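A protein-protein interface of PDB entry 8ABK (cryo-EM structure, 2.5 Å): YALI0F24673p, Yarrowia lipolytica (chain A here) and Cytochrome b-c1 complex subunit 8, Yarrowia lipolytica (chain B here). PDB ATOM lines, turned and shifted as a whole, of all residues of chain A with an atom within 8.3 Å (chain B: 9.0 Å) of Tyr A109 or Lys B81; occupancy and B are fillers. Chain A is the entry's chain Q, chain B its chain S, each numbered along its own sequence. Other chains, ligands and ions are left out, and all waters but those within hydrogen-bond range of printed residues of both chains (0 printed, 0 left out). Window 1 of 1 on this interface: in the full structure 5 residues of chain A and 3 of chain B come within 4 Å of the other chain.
No residue of chain B comes within 4 Å of Glu A108. Printed residues of chain B within 4 Å of Tyr A109: Lys B81 (3.4 Å) and Arg B84 (3.4 Å). Of the printed residues of chain B, Glu A111 touches Lys B81 (2.7 Å). Of the printed residues of chain B, Glu A115 touches Thr B80 (3.3 Å) and Lys B81 (2.8 Å). Of the printed residues of chain B, Glu A116 touches Lys B81 (2.8 Å). Printed residues of chain A within 4 Å of Thr B80: Glu A115 (3.3 Å). Of the printed residues of chain A, Lys B81 touches Tyr A109, Glu A111, Asp A112, Glu A115 and Glu A116. No residue of chain A comes within 4 Å of Ala B82. Of the printed residues of chain A, Arg B84 touches Tyr A109 (3.4 Å). The nearest printed residue of chain B that does not touch Glu A111 is Arg B84 (6.9 Å).
Printed residues of chain A that touch a printed residue of chain B: Tyr A109, Glu A111, Asp A112, Glu A115 and Glu A116. Of the 12 printed residues of chain B, 3 touch a printed residue of chain A. Printed residues of chain B that touch a printed residue of chain A: Thr B80, Lys B81 and Arg B84. Among the printed residues, Asp or Glu carboxylates within 4 Å of a Lys or Arg side-chain nitrogen of the other chain: Glu A111 with Lys B81 and Glu A116 with Lys B81.
The side-chain carboxylate (OE1) of Glu A116 is in salt-bridge range of the side-chain amino group (NZ) of Lys B81. OE2 of Glu A115 is in hydrogen-bond range of N of Lys B81 (2.8 Å). The side-chain carboxylate (OE1) of Glu A111 lies within salt-bridge range of the side-chain amino group (NZ) of Lys B81 (2.7 Å).
CD of Lys B81 touches OH of Tyr A109, at 3.4 Å. Arg B84 touches Tyr A109. Asp A112 touches Lys B81 (O to NZ, 3.6 Å). Glu A115 touches Thr B80.
The guanidinium group (NH1) of Arg A94 lies within salt-bridge range of the side-chain carboxylate (OE2) of Glu A111 (3.1 Å). SG of Cys A91 is disulfide-bonded to SG of Cys A113 (2.1 Å). O of Trp B77 lies within hydrogen-bond range of OG1 of Thr B80, 2.6 Å away. The side-chain carboxylate of Asp A112 sits at hydrogen-bond distance from the backbone NH of Val A114 (3.0 Å).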
ATOM      1  N   HIS A  87       8.448 -11.988 -22.550  1.00  0.00           N
ATOM      2  CA  HIS A  87       7.678 -13.060 -21.939  1.00  0.00           C
ATOM      3  C   HIS A  87       6.328 -12.525 -21.475  1.00  0.00           C
ATOM      4  O   HIS A  87       5.310 -13.172 -21.712  1.00  0.00           O
ATOM      5  CB  HIS A  87       8.455 -13.740 -20.809  1.00  0.00           C
ATOM      6  CG  HIS A  87       9.683 -14.451 -21.268  1.00  0.00           C
ATOM      7  ND1 HIS A  87      10.772 -14.631 -20.443  1.00  0.00           N
ATOM      8  CD2 HIS A  87      10.011 -15.013 -22.452  1.00  0.00           C
ATOM      9  CE1 HIS A  87      11.717 -15.280 -21.096  1.00  0.00           C
ATOM     10  NE2 HIS A  87      11.274 -15.521 -22.333  1.00  0.00           N
ATOM     11  N   GLU A  90       4.193 -11.855 -24.615  1.00  0.00           N
ATOM     12  CA  GLU A  90       3.657 -13.099 -25.145  1.00  0.00           C
ATOM     13  C   GLU A  90       2.499 -13.584 -24.276  1.00  0.00           C
ATOM     14  O   GLU A  90       1.464 -13.989 -24.803  1.00  0.00           O
ATOM     15  CB  GLU A  90       4.668 -14.224 -25.051  1.00  0.00           C
ATOM     16  CG  GLU A  90       5.339 -14.527 -26.355  1.00  0.00           C
ATOM     17  CD  GLU A  90       6.808 -14.665 -26.041  1.00  0.00           C
ATOM     18  OE1 GLU A  90       7.135 -15.291 -25.003  1.00  0.00           O
ATOM     19  OE2 GLU A  90       7.624 -14.112 -26.800  1.00  0.00           O
ATOM     20  N   CYS A  91       2.695 -13.550 -22.950  1.00  0.00           N
ATOM     21  CA  CYS A  91       1.671 -13.984 -22.015  1.00  0.00           C
ATOM     22  C   CYS A  91       0.390 -13.181 -22.232  1.00  0.00           C
ATOM     23  O   CYS A  91      -0.671 -13.788 -22.373  1.00  0.00           O
ATOM     24  CB  CYS A  91       2.131 -13.872 -20.568  1.00  0.00           C
ATOM     25  SG  CYS A  91       0.911 -14.451 -19.355  1.00  0.00           S
ATOM     26  N   VAL A  92       0.486 -11.839 -22.280  1.00  0.00           N
ATOM     27  CA  VAL A  92      -0.719 -11.031 -22.423  1.00  0.00           C
ATOM     28  C   VAL A  92      -1.447 -11.383 -23.716  1.00  0.00           C
ATOM     29  O   VAL A  92      -2.660 -11.578 -23.677  1.00  0.00           O
ATOM     30  CB  VAL A  92      -0.544  -9.518 -22.194  1.00  0.00           C
ATOM     31  CG1 VAL A  92       0.051  -9.191 -20.838  1.00  0.00           C
ATOM     32  CG2 VAL A  92       0.215  -8.835 -23.308  1.00  0.00           C
ATOM     33  N   ARG A  94      -1.553 -14.225 -25.295  1.00  0.00           N
ATOM     34  CA  ARG A  94      -2.214 -15.514 -25.116  1.00  0.00           C
ATOM     35  C   ARG A  94      -3.478 -15.361 -24.280  1.00  0.00           C
ATOM     36  O   ARG A  94      -4.501 -15.955 -24.613  1.00  0.00           O
ATOM     37  CB  ARG A  94      -1.300 -16.563 -24.478  1.00  0.00           C
ATOM     38  CG  ARG A  94      -0.079 -16.902 -25.319  1.00  0.00           C
ATOM     39  CD  ARG A  94       0.924 -17.853 -24.701  1.00  0.00           C
ATOM     40  NE  ARG A  94       1.578 -17.368 -23.487  1.00  0.00           N
ATOM     41  CZ  ARG A  94       1.446 -17.940 -22.296  1.00  0.00           C
ATOM     42  NH1 ARG A  94       0.697 -19.023 -22.173  1.00  0.00           N
ATOM     43  NH2 ARG A  94       2.086 -17.436 -21.255  1.00  0.00           N
ATOM     44  N   VAL A  95      -3.395 -14.581 -23.199  1.00  0.00           N
ATOM     45  CA  VAL A  95      -4.476 -14.530 -22.231  1.00  0.00           C
ATOM     46  C   VAL A  95      -5.648 -13.751 -22.823  1.00  0.00           C
ATOM     47  O   VAL A  95      -6.787 -14.191 -22.702  1.00  0.00           O
ATOM     48  CB  VAL A  95      -3.998 -14.024 -20.855  1.00  0.00           C
ATOM     49  CG1 VAL A  95      -5.153 -13.652 -19.935  1.00  0.00           C
ATOM     50  CG2 VAL A  95      -3.102 -15.059 -20.182  1.00  0.00           C
ATOM     51  N   ALA A  98      -7.372 -15.817 -25.235  1.00  0.00           N
ATOM     52  CA  ALA A  98      -8.076 -16.900 -24.574  1.00  0.00           C
ATOM     53  C   ALA A  98      -9.377 -16.370 -23.983  1.00  0.00           C
ATOM     54  O   ALA A  98     -10.348 -17.110 -23.881  1.00  0.00           O
ATOM     55  CB  ALA A  98      -7.192 -17.529 -23.527  1.00  0.00           C
ATOM     56  N   ASP A 103     -16.776 -19.694 -24.014  1.00  0.00           N
ATOM     57  CA  ASP A 103     -16.706 -20.717 -22.979  1.00  0.00           C
ATOM     58  C   ASP A 103     -15.380 -20.612 -22.225  1.00  0.00           C
ATOM     59  O   ASP A 103     -14.830 -21.618 -21.772  1.00  0.00           O
ATOM     60  CB  ASP A 103     -17.023 -22.117 -23.518  1.00  0.00           C
ATOM     61  CG  ASP A 103     -18.257 -22.173 -24.404  1.00  0.00           C
ATOM     62  OD1 ASP A 103     -19.316 -21.671 -23.976  1.00  0.00           O
ATOM     63  OD2 ASP A 103     -18.148 -22.720 -25.520  1.00  0.00           O
ATOM     64  N   TYR A 104     -14.880 -19.375 -22.112  1.00  0.00           N
ATOM     65  CA  TYR A 104     -13.732 -19.060 -21.282  1.00  0.00           C
ATOM     66  C   TYR A 104     -14.183 -18.926 -19.830  1.00  0.00           C
ATOM     67  O   TYR A 104     -13.445 -19.286 -18.915  1.00  0.00           O
ATOM     68  CB  TYR A 104     -13.041 -17.781 -21.762  1.00  0.00           C
ATOM     69  CG  TYR A 104     -12.070 -17.191 -20.769  1.00  0.00           C
ATOM     70  CD1 TYR A 104     -10.802 -17.730 -20.598  1.00  0.00           C
ATOM     71  CD2 TYR A 104     -12.431 -16.116 -19.969  1.00  0.00           C
ATOM     72  CE1 TYR A 104      -9.913 -17.208 -19.668  1.00  0.00           C
ATOM     73  CE2 TYR A 104     -11.557 -15.586 -19.032  1.00  0.00           C
ATOM     74  CZ  TYR A 104     -10.290 -16.128 -18.885  1.00  0.00           C
ATOM     75  OH  TYR A 104      -9.420 -15.596 -17.977  1.00  0.00           O
ATOM     76  N   ASP A 105     -15.398 -18.395 -19.643  1.00  0.00           N
ATOM     77  CA  ASP A 105     -15.952 -18.131 -18.325  1.00  0.00           C
ATOM     78  C   ASP A 105     -16.249 -19.448 -17.610  1.00  0.00           C
ATOM     79  O   ASP A 105     -16.221 -19.501 -16.383  1.00  0.00           O
ATOM     80  CB  ASP A 105     -17.168 -17.203 -18.402  1.00  0.00           C
ATOM     81  CG  ASP A 105     -18.275 -17.702 -19.317  1.00  0.00           C
ATOM     82  OD1 ASP A 105     -17.956 -18.169 -20.433  1.00  0.00           O
ATOM     83  OD2 ASP A 105     -19.451 -17.617 -18.908  1.00  0.00           O
ATOM     84  N   HIS A 106     -16.516 -20.500 -18.400  1.00  0.00           N
ATOM     85  CA  HIS A 106     -16.773 -21.838 -17.891  1.00  0.00           C
ATOM     86  C   HIS A 106     -15.552 -22.730 -18.113  1.00  0.00           C
ATOM     87  O   HIS A 106     -15.681 -23.882 -18.527  1.00  0.00           O
ATOM     88  CB  HIS A 106     -18.056 -22.416 -18.508  1.00  0.00           C
ATOM     89  CG  HIS A 106     -19.293 -21.680 -18.117  1.00  0.00           C
ATOM     90  ND1 HIS A 106     -19.841 -21.773 -16.852  1.00  0.00           N
ATOM     91  CD2 HIS A 106     -20.088 -20.841 -18.814  1.00  0.00           C
ATOM     92  CE1 HIS A 106     -20.922 -21.022 -16.787  1.00  0.00           C
ATOM     93  NE2 HIS A 106     -21.095 -20.438 -17.979  1.00  0.00           N
ATOM     94  N   ALA A 107     -14.366 -22.177 -17.835  1.00  0.00           N
ATOM     95  CA  ALA A 107     -13.129 -22.940 -17.850  1.00  0.00           C
ATOM     96  C   ALA A 107     -12.669 -23.162 -16.412  1.00  0.00           C
ATOM     97  O   ALA A 107     -13.057 -22.424 -15.502  1.00  0.00           O
ATOM     98  CB  ALA A 107     -12.089 -22.246 -18.702  1.00  0.00           C
ATOM     99  N   GLU A 108     -11.871 -24.213 -16.215  1.00  0.00           N
ATOM    100  CA  GLU A 108     -11.434 -24.585 -14.883  1.00  0.00           C
ATOM    101  C   GLU A 108     -10.277 -23.670 -14.496  1.00  0.00           C
ATOM    102  O   GLU A 108     -10.321 -23.015 -13.451  1.00  0.00           O
ATOM    103  CB  GLU A 108     -11.082 -26.076 -14.858  1.00  0.00           C
ATOM    104  CG  GLU A 108     -10.923 -26.662 -13.460  1.00  0.00           C
ATOM    105  CD  GLU A 108      -9.596 -26.395 -12.763  1.00  0.00           C
ATOM    106  OE1 GLU A 108      -9.619 -25.824 -11.652  1.00  0.00           O
ATOM    107  OE2 GLU A 108      -8.543 -26.770 -13.324  1.00  0.00           O
ATOM    108  N   TYR A 109      -9.273 -23.625 -15.382  1.00  0.00           N
ATOM    109  CA  TYR A 109      -8.060 -22.858 -15.172  1.00  0.00           C
ATOM    110  C   TYR A 109      -8.040 -21.641 -16.092  1.00  0.00           C
ATOM    111  O   TYR A 109      -7.974 -21.778 -17.310  1.00  0.00           O
ATOM    112  CB  TYR A 109      -6.815 -23.724 -15.398  1.00  0.00           C
ATOM    113  CG  TYR A 109      -5.514 -22.961 -15.342  1.00  0.00           C
ATOM    114  CD1 TYR A 109      -5.108 -22.327 -14.173  1.00  0.00           C
ATOM    115  CD2 TYR A 109      -4.692 -22.855 -16.456  1.00  0.00           C
ATOM    116  CE1 TYR A 109      -3.919 -21.619 -14.108  1.00  0.00           C
ATOM    117  CE2 TYR A 109      -3.495 -22.155 -16.407  1.00  0.00           C
ATOM    118  CZ  TYR A 109      -3.103 -21.546 -15.224  1.00  0.00           C
ATOM    119  OH  TYR A 109      -1.927 -20.854 -15.156  1.00  0.00           O
ATOM    120  N   LYS A 110      -8.069 -20.455 -15.480  1.00  0.00           N
ATOM    121  CA  LYS A 110      -7.821 -19.215 -16.190  1.00  0.00           C
ATOM    122  C   LYS A 110      -6.411 -18.725 -15.862  1.00  0.00           C
ATOM    123  O   LYS A 110      -6.097 -18.420 -14.711  1.00  0.00           O
ATOM    124  CB  LYS A 110      -8.908 -18.201 -15.833  1.00  0.00           C
ATOM    125  CG  LYS A 110     -10.338 -18.599 -16.193  1.00  0.00           C
ATOM    126  CD  LYS A 110     -11.354 -17.729 -15.463  1.00  0.00           C
ATOM    127  CE  LYS A 110     -12.798 -17.945 -15.868  1.00  0.00           C
ATOM    128  NZ  LYS A 110     -13.340 -19.250 -15.416  1.00  0.00           N
ATOM    129  N   GLU A 111      -5.565 -18.682 -16.894  1.00  0.00           N
ATOM    130  CA  GLU A 111      -4.210 -18.170 -16.782  1.00  0.00           C
ATOM    131  C   GLU A 111      -4.229 -16.650 -16.608  1.00  0.00           C
ATOM    132  O   GLU A 111      -4.998 -15.964 -17.284  1.00  0.00           O
ATOM    133  CB  GLU A 111      -3.451 -18.520 -18.056  1.00  0.00           C
ATOM    134  CG  GLU A 111      -1.960 -18.573 -17.850  1.00  0.00           C
ATOM    135  CD  GLU A 111      -1.119 -18.578 -19.111  1.00  0.00           C
ATOM    136  OE1 GLU A 111       0.065 -18.232 -18.994  1.00  0.00           O
ATOM    137  OE2 GLU A 111      -1.636 -18.936 -20.198  1.00  0.00           O
ATOM    138  N   ASP A 112      -3.347 -16.136 -15.725  1.00  0.00           N
ATOM    139  CA  ASP A 112      -3.033 -14.715 -15.658  1.00  0.00           C
ATOM    140  C   ASP A 112      -1.596 -14.487 -16.115  1.00  0.00           C
ATOM    141  O   ASP A 112      -0.921 -15.427 -16.528  1.00  0.00           O
ATOM    142  CB  ASP A 112      -3.254 -14.133 -14.261  1.00  0.00           C
ATOM    143  CG  ASP A 112      -2.523 -14.888 -13.165  1.00  0.00           C
ATOM    144  OD1 ASP A 112      -1.318 -14.631 -12.950  1.00  0.00           O
ATOM    145  OD2 ASP A 112      -3.156 -15.780 -12.576  1.00  0.00           O
ATOM    146  N   CYS A 113      -1.151 -13.231 -16.012  1.00  0.00           N
ATOM    147  CA  CYS A 113       0.208 -12.874 -16.382  1.00  0.00           C
ATOM    148  C   CYS A 113       0.954 -12.235 -15.219  1.00  0.00           C
ATOM    149  O   CYS A 113       1.973 -11.571 -15.418  1.00  0.00           O
ATOM    150  CB  CYS A 113       0.200 -11.972 -17.603  1.00  0.00           C
ATOM    151  SG  CYS A 113      -0.403 -12.889 -19.040  1.00  0.00           S
ATOM    152  N   VAL A 114       0.483 -12.526 -14.009  1.00  0.00           N
ATOM    153  CA  VAL A 114       1.066 -11.927 -12.828  1.00  0.00           C
ATOM    154  C   VAL A 114       2.515 -12.379 -12.677  1.00  0.00           C
ATOM    155  O   VAL A 114       3.391 -11.550 -12.442  1.00  0.00           O
ATOM    156  CB  VAL A 114       0.197 -12.201 -11.589  1.00  0.00           C
ATOM    157  CG1 VAL A 114       0.947 -11.970 -10.288  1.00  0.00           C
ATOM    158  CG2 VAL A 114      -1.042 -11.340 -11.637  1.00  0.00           C
ATOM    159  N   GLU A 115       2.767 -13.680 -12.867  1.00  0.00           N
ATOM    160  CA  GLU A 115       4.110 -14.210 -12.693  1.00  0.00           C
ATOM    161  C   GLU A 115       5.107 -13.464 -13.573  1.00  0.00           C
ATOM    162  O   GLU A 115       6.148 -13.022 -13.097  1.00  0.00           O
ATOM    163  CB  GLU A 115       4.168 -15.696 -13.025  1.00  0.00           C
ATOM    164  CG  GLU A 115       4.246 -16.571 -11.796  1.00  0.00           C
ATOM    165  CD  GLU A 115       4.151 -18.063 -12.070  1.00  0.00           C
ATOM    166  OE1 GLU A 115       5.026 -18.597 -12.788  1.00  0.00           O
ATOM    167  OE2 GLU A 115       3.197 -18.691 -11.565  1.00  0.00           O
ATOM    168  N   GLU A 116       4.765 -13.322 -14.857  1.00  0.00           N
ATOM    169  CA  GLU A 116       5.658 -12.741 -15.847  1.00  0.00           C
ATOM    170  C   GLU A 116       5.834 -11.256 -15.571  1.00  0.00           C
ATOM    171  O   GLU A 116       6.899 -10.688 -15.823  1.00  0.00           O
ATOM    172  CB  GLU A 116       5.059 -12.894 -17.244  1.00  0.00           C
ATOM    173  CG  GLU A 116       5.241 -14.271 -17.829  1.00  0.00           C
ATOM    174  CD  GLU A 116       4.178 -15.280 -17.423  1.00  0.00           C
ATOM    175  OE1 GLU A 116       4.265 -16.420 -17.889  1.00  0.00           O
ATOM    176  OE2 GLU A 116       3.299 -14.937 -16.603  1.00  0.00           O
ATOM    177  N   PHE A 117       4.752 -10.643 -15.093  1.00  0.00           N
ATOM    178  CA  PHE A 117       4.774  -9.245 -14.725  1.00  0.00           C
ATOM    179  C   PHE A 117       5.734  -9.044 -13.556  1.00  0.00           C
ATOM    180  O   PHE A 117       6.581  -8.150 -13.610  1.00  0.00           O
ATOM    181  CB  PHE A 117       3.351  -8.792 -14.417  1.00  0.00           C
ATOM    182  CG  PHE A 117       3.266  -7.327 -14.107  1.00  0.00           C
ATOM    183  CD1 PHE A 117       3.438  -6.383 -15.110  1.00  0.00           C
ATOM    184  CD2 PHE A 117       3.047  -6.895 -12.808  1.00  0.00           C
ATOM    185  CE1 PHE A 117       3.372  -5.028 -14.816  1.00  0.00           C
ATOM    186  CE2 PHE A 117       2.970  -5.539 -12.520  1.00  0.00           C
ATOM    187  CZ  PHE A 117       3.128  -4.609 -13.526  1.00  0.00           C
ATOM    188  N   HIS A 119       8.261 -10.930 -12.853  1.00  0.00           N
ATOM    189  CA  HIS A 119       9.633 -11.131 -13.306  1.00  0.00           C
ATOM    190  C   HIS A 119      10.172  -9.876 -13.986  1.00  0.00           C
ATOM    191  O   HIS A 119      11.331  -9.506 -13.788  1.00  0.00           O
ATOM    192  CB  HIS A 119       9.781 -12.381 -14.170  1.00  0.00           C
ATOM    193  CG  HIS A 119       9.480 -13.631 -13.422  1.00  0.00           C
ATOM    194  ND1 HIS A 119       9.859 -13.810 -12.104  1.00  0.00           N
ATOM    195  CD2 HIS A 119       8.845 -14.760 -13.796  1.00  0.00           C
ATOM    196  CE1 HIS A 119       9.455 -14.992 -11.694  1.00  0.00           C
ATOM    197  NE2 HIS A 119       8.833 -15.599 -12.714  1.00  0.00           N
ATOM    198  N   GLU B  76       9.046 -23.470  -4.047  1.00  0.00           N
ATOM    199  CA  GLU B  76       8.875 -22.298  -4.885  1.00  0.00           C
ATOM    200  C   GLU B  76       8.264 -22.698  -6.226  1.00  0.00           C
ATOM    201  O   GLU B  76       7.407 -21.993  -6.749  1.00  0.00           O
ATOM    202  CB  GLU B  76      10.206 -21.567  -5.060  1.00  0.00           C
ATOM    203  CG  GLU B  76      10.230 -20.595  -6.225  1.00  0.00           C
ATOM    204  CD  GLU B  76      11.387 -19.607  -6.245  1.00  0.00           C
ATOM    205  OE1 GLU B  76      11.846 -19.190  -5.155  1.00  0.00           O
ATOM    206  OE2 GLU B  76      11.829 -19.249  -7.357  1.00  0.00           O
ATOM    207  N   TRP B  77       8.735 -23.821  -6.766  1.00  0.00           N
ATOM    208  CA  TRP B  77       8.368 -24.259  -8.095  1.00  0.00           C
ATOM    209  C   TRP B  77       6.935 -24.780  -8.107  1.00  0.00           C
ATOM    210  O   TRP B  77       6.230 -24.644  -9.101  1.00  0.00           O
ATOM    211  CB  TRP B  77       9.354 -25.322  -8.572  1.00  0.00           C
ATOM    212  CG  TRP B  77       9.007 -25.789  -9.946  1.00  0.00           C
ATOM    213  CD1 TRP B  77       9.274 -25.148 -11.121  1.00  0.00           C
ATOM    214  CD2 TRP B  77       8.260 -26.965 -10.286  1.00  0.00           C
ATOM    215  NE1 TRP B  77       8.777 -25.862 -12.176  1.00  0.00           N
ATOM    216  CE2 TRP B  77       8.147 -26.979 -11.696  1.00  0.00           C
ATOM    217  CE3 TRP B  77       7.693 -28.005  -9.540  1.00  0.00           C
ATOM    218  CZ2 TRP B  77       7.483 -27.998 -12.376  1.00  0.00           C
ATOM    219  CZ3 TRP B  77       7.054 -29.022 -10.217  1.00  0.00           C
ATOM    220  CH2 TRP B  77       6.954 -29.013 -11.613  1.00  0.00           C
ATOM    221  N   LEU B  78       6.513 -25.372  -6.991  1.00  0.00           N
ATOM    222  CA  LEU B  78       5.195 -25.976  -6.934  1.00  0.00           C
ATOM    223  C   LEU B  78       4.122 -24.895  -6.968  1.00  0.00           C
ATOM    224  O   LEU B  78       2.993 -25.173  -7.351  1.00  0.00           O
ATOM    225  CB  LEU B  78       5.077 -26.788  -5.643  1.00  0.00           C
ATOM    226  CG  LEU B  78       5.681 -28.188  -5.680  1.00  0.00           C
ATOM    227  CD1 LEU B  78       5.624 -28.835  -4.306  1.00  0.00           C
ATOM    228  CD2 LEU B  78       4.951 -29.052  -6.689  1.00  0.00           C
ATOM    229  N   TYR B  79       4.478 -23.675  -6.554  1.00  0.00           N
ATOM    230  CA  TYR B  79       3.510 -22.595  -6.473  1.00  0.00           C
ATOM    231  C   TYR B  79       3.663 -21.627  -7.639  1.00  0.00           C
ATOM    232  O   TYR B  79       3.205 -20.492  -7.565  1.00  0.00           O
ATOM    233  CB  TYR B  79       3.585 -21.916  -5.107  1.00  0.00           C
ATOM    234  CG  TYR B  79       2.959 -22.767  -4.041  1.00  0.00           C
ATOM    235  CD1 TYR B  79       1.614 -22.644  -3.736  1.00  0.00           C
ATOM    236  CD2 TYR B  79       3.698 -23.742  -3.386  1.00  0.00           C
ATOM    237  CE1 TYR B  79       1.021 -23.451  -2.778  1.00  0.00           C
ATOM    238  CE2 TYR B  79       3.119 -24.563  -2.431  1.00  0.00           C
ATOM    239  CZ  TYR B  79       1.774 -24.417  -2.129  1.00  0.00           C
ATOM    240  OH  TYR B  79       1.195 -25.218  -1.190  1.00  0.00           O
ATOM    241  N   THR B  80       4.315 -22.085  -8.707  1.00  0.00           N
ATOM    242  CA  THR B  80       4.271 -21.392  -9.982  1.00  0.00           C
ATOM    243  C   THR B  80       3.202 -22.045 -10.850  1.00  0.00           C
ATOM    244  O   THR B  80       2.595 -23.035 -10.438  1.00  0.00           O
ATOM    245  CB  THR B  80       5.653 -21.381 -10.638  1.00  0.00           C
ATOM    246  OG1 THR B  80       6.032 -22.729 -10.914  1.00  0.00           O
ATOM    247  CG2 THR B  80       6.697 -20.725  -9.766  1.00  0.00           C
ATOM    248  N   LYS B  81       2.977 -21.460 -12.034  1.00  0.00           N
ATOM    249  CA  LYS B  81       2.028 -21.952 -13.016  1.00  0.00           C
ATOM    250  C   LYS B  81       2.494 -23.306 -13.533  1.00  0.00           C
ATOM    251  O   LYS B  81       1.691 -24.220 -13.695  1.00  0.00           O
ATOM    252  CB  LYS B  81       1.972 -21.001 -14.212  1.00  0.00           C
ATOM    253  CG  LYS B  81       1.127 -19.756 -14.012  1.00  0.00           C
ATOM    254  CD  LYS B  81       0.870 -18.990 -15.299  1.00  0.00           C
ATOM    255  CE  LYS B  81       2.006 -18.074 -15.705  1.00  0.00           C
ATOM    256  NZ  LYS B  81       1.879 -17.639 -17.116  1.00  0.00           N
ATOM    257  N   ALA B  82       3.804 -23.403 -13.797  1.00  0.00           N
ATOM    258  CA  ALA B  82       4.463 -24.606 -14.282  1.00  0.00           C
ATOM    259  C   ALA B  82       4.265 -25.783 -13.326  1.00  0.00           C
ATOM    260  O   ALA B  82       4.252 -26.938 -13.759  1.00  0.00           O
ATOM    261  CB  ALA B  82       5.929 -24.317 -14.487  1.00  0.00           C
ATOM    262  N   GLY B  83       4.127 -25.483 -12.029  1.00  0.00           N
ATOM    263  CA  GLY B  83       4.100 -26.516 -11.009  1.00  0.00           C
ATOM    264  C   GLY B  83       2.688 -26.869 -10.556  1.00  0.00           C
ATOM    265  O   GLY B  83       2.527 -27.519  -9.522  1.00  0.00           O
ATOM    266  N   ARG B  84       1.691 -26.424 -11.333  1.00  0.00           N
ATOM    267  CA  ARG B  84       0.281 -26.538 -10.997  1.00  0.00           C
ATOM    268  C   ARG B  84      -0.103 -27.992 -10.783  1.00  0.00           C
ATOM    269  O   ARG B  84      -0.843 -28.309  -9.857  1.00  0.00           O
ATOM    270  CB  ARG B  84      -0.572 -26.152 -12.198  1.00  0.00           C
ATOM    271  CG  ARG B  84      -1.001 -24.697 -12.195  1.00  0.00           C
ATOM    272  CD  ARG B  84      -2.166 -24.570 -13.134  1.00  0.00           C
ATOM    273  NE  ARG B  84      -1.739 -24.732 -14.512  1.00  0.00           N
ATOM    274  CZ  ARG B  84      -2.471 -25.326 -15.441  1.00  0.00           C
ATOM    275  NH1 ARG B  84      -3.666 -25.807 -15.138  1.00  0.00           N
ATOM    276  NH2 ARG B  84      -2.014 -25.420 -16.676  1.00  0.00           N
ATOM    277  N   HIS B  85       0.364 -28.839 -11.706  1.00  0.00           N
ATOM    278  CA  HIS B  85      -0.084 -30.212 -11.799  1.00  0.00           C
ATOM    279  C   HIS B  85       0.550 -31.034 -10.691  1.00  0.00           C
ATOM    280  O   HIS B  85      -0.105 -31.883 -10.092  1.00  0.00           O
ATOM    281  CB  HIS B  85       0.299 -30.793 -13.158  1.00  0.00           C
ATOM    282  CG  HIS B  85      -0.296 -30.032 -14.286  1.00  0.00           C
ATOM    283  ND1 HIS B  85      -1.661 -29.903 -14.445  1.00  0.00           N
ATOM    284  CD2 HIS B  85       0.277 -29.352 -15.298  1.00  0.00           C
ATOM    285  CE1 HIS B  85      -1.906 -29.185 -15.521  1.00  0.00           C
ATOM    286  NE2 HIS B  85      -0.732 -28.835 -16.063  1.00  0.00           N
ATOM    287  N   GLU B  86       1.843 -30.775 -10.471  1.00  0.00           N
ATOM    288  CA  GLU B  86       2.610 -31.455  -9.446  1.00  0.00           C
ATOM    289  C   GLU B  86       2.099 -31.011  -8.083  1.00  0.00           C
ATOM    290  O   GLU B  86       2.172 -31.786  -7.133  1.00  0.00           O
ATOM    291  CB  GLU B  86       4.109 -31.185  -9.589  1.00  0.00           C
ATOM    292  CG  GLU B  86       4.777 -31.938 -10.728  1.00  0.00           C
ATOM    293  CD  GLU B  86       4.445 -31.483 -12.143  1.00  0.00           C
ATOM    294  OE1 GLU B  86       4.099 -30.294 -12.332  1.00  0.00           O
ATOM    295  OE2 GLU B  86       4.513 -32.331 -13.055  1.00  0.00           O
ATOM    296  N   LEU B  87       1.600 -29.766  -8.000  1.00  0.00           N
ATOM    297  CA  LEU B  87       1.074 -29.276  -6.735  1.00  0.00           C
ATOM    298  C   LEU B  87      -0.253 -29.963  -6.434  1.00  0.00           C
ATOM    299  O   LEU B  87      -0.568 -30.222  -5.276  1.00  0.00           O
ATOM    300  CB  LEU B  87       0.921 -27.748  -6.726  1.00  0.00           C
ATOM    301  CG  LEU B  87       0.313 -27.148  -5.449  1.00  0.00           C
ATOM    302  CD1 LEU B  87       1.228 -27.332  -4.241  1.00  0.00           C
ATOM    303  CD2 LEU B  87      -0.006 -25.675  -5.632  1.00  0.00           C
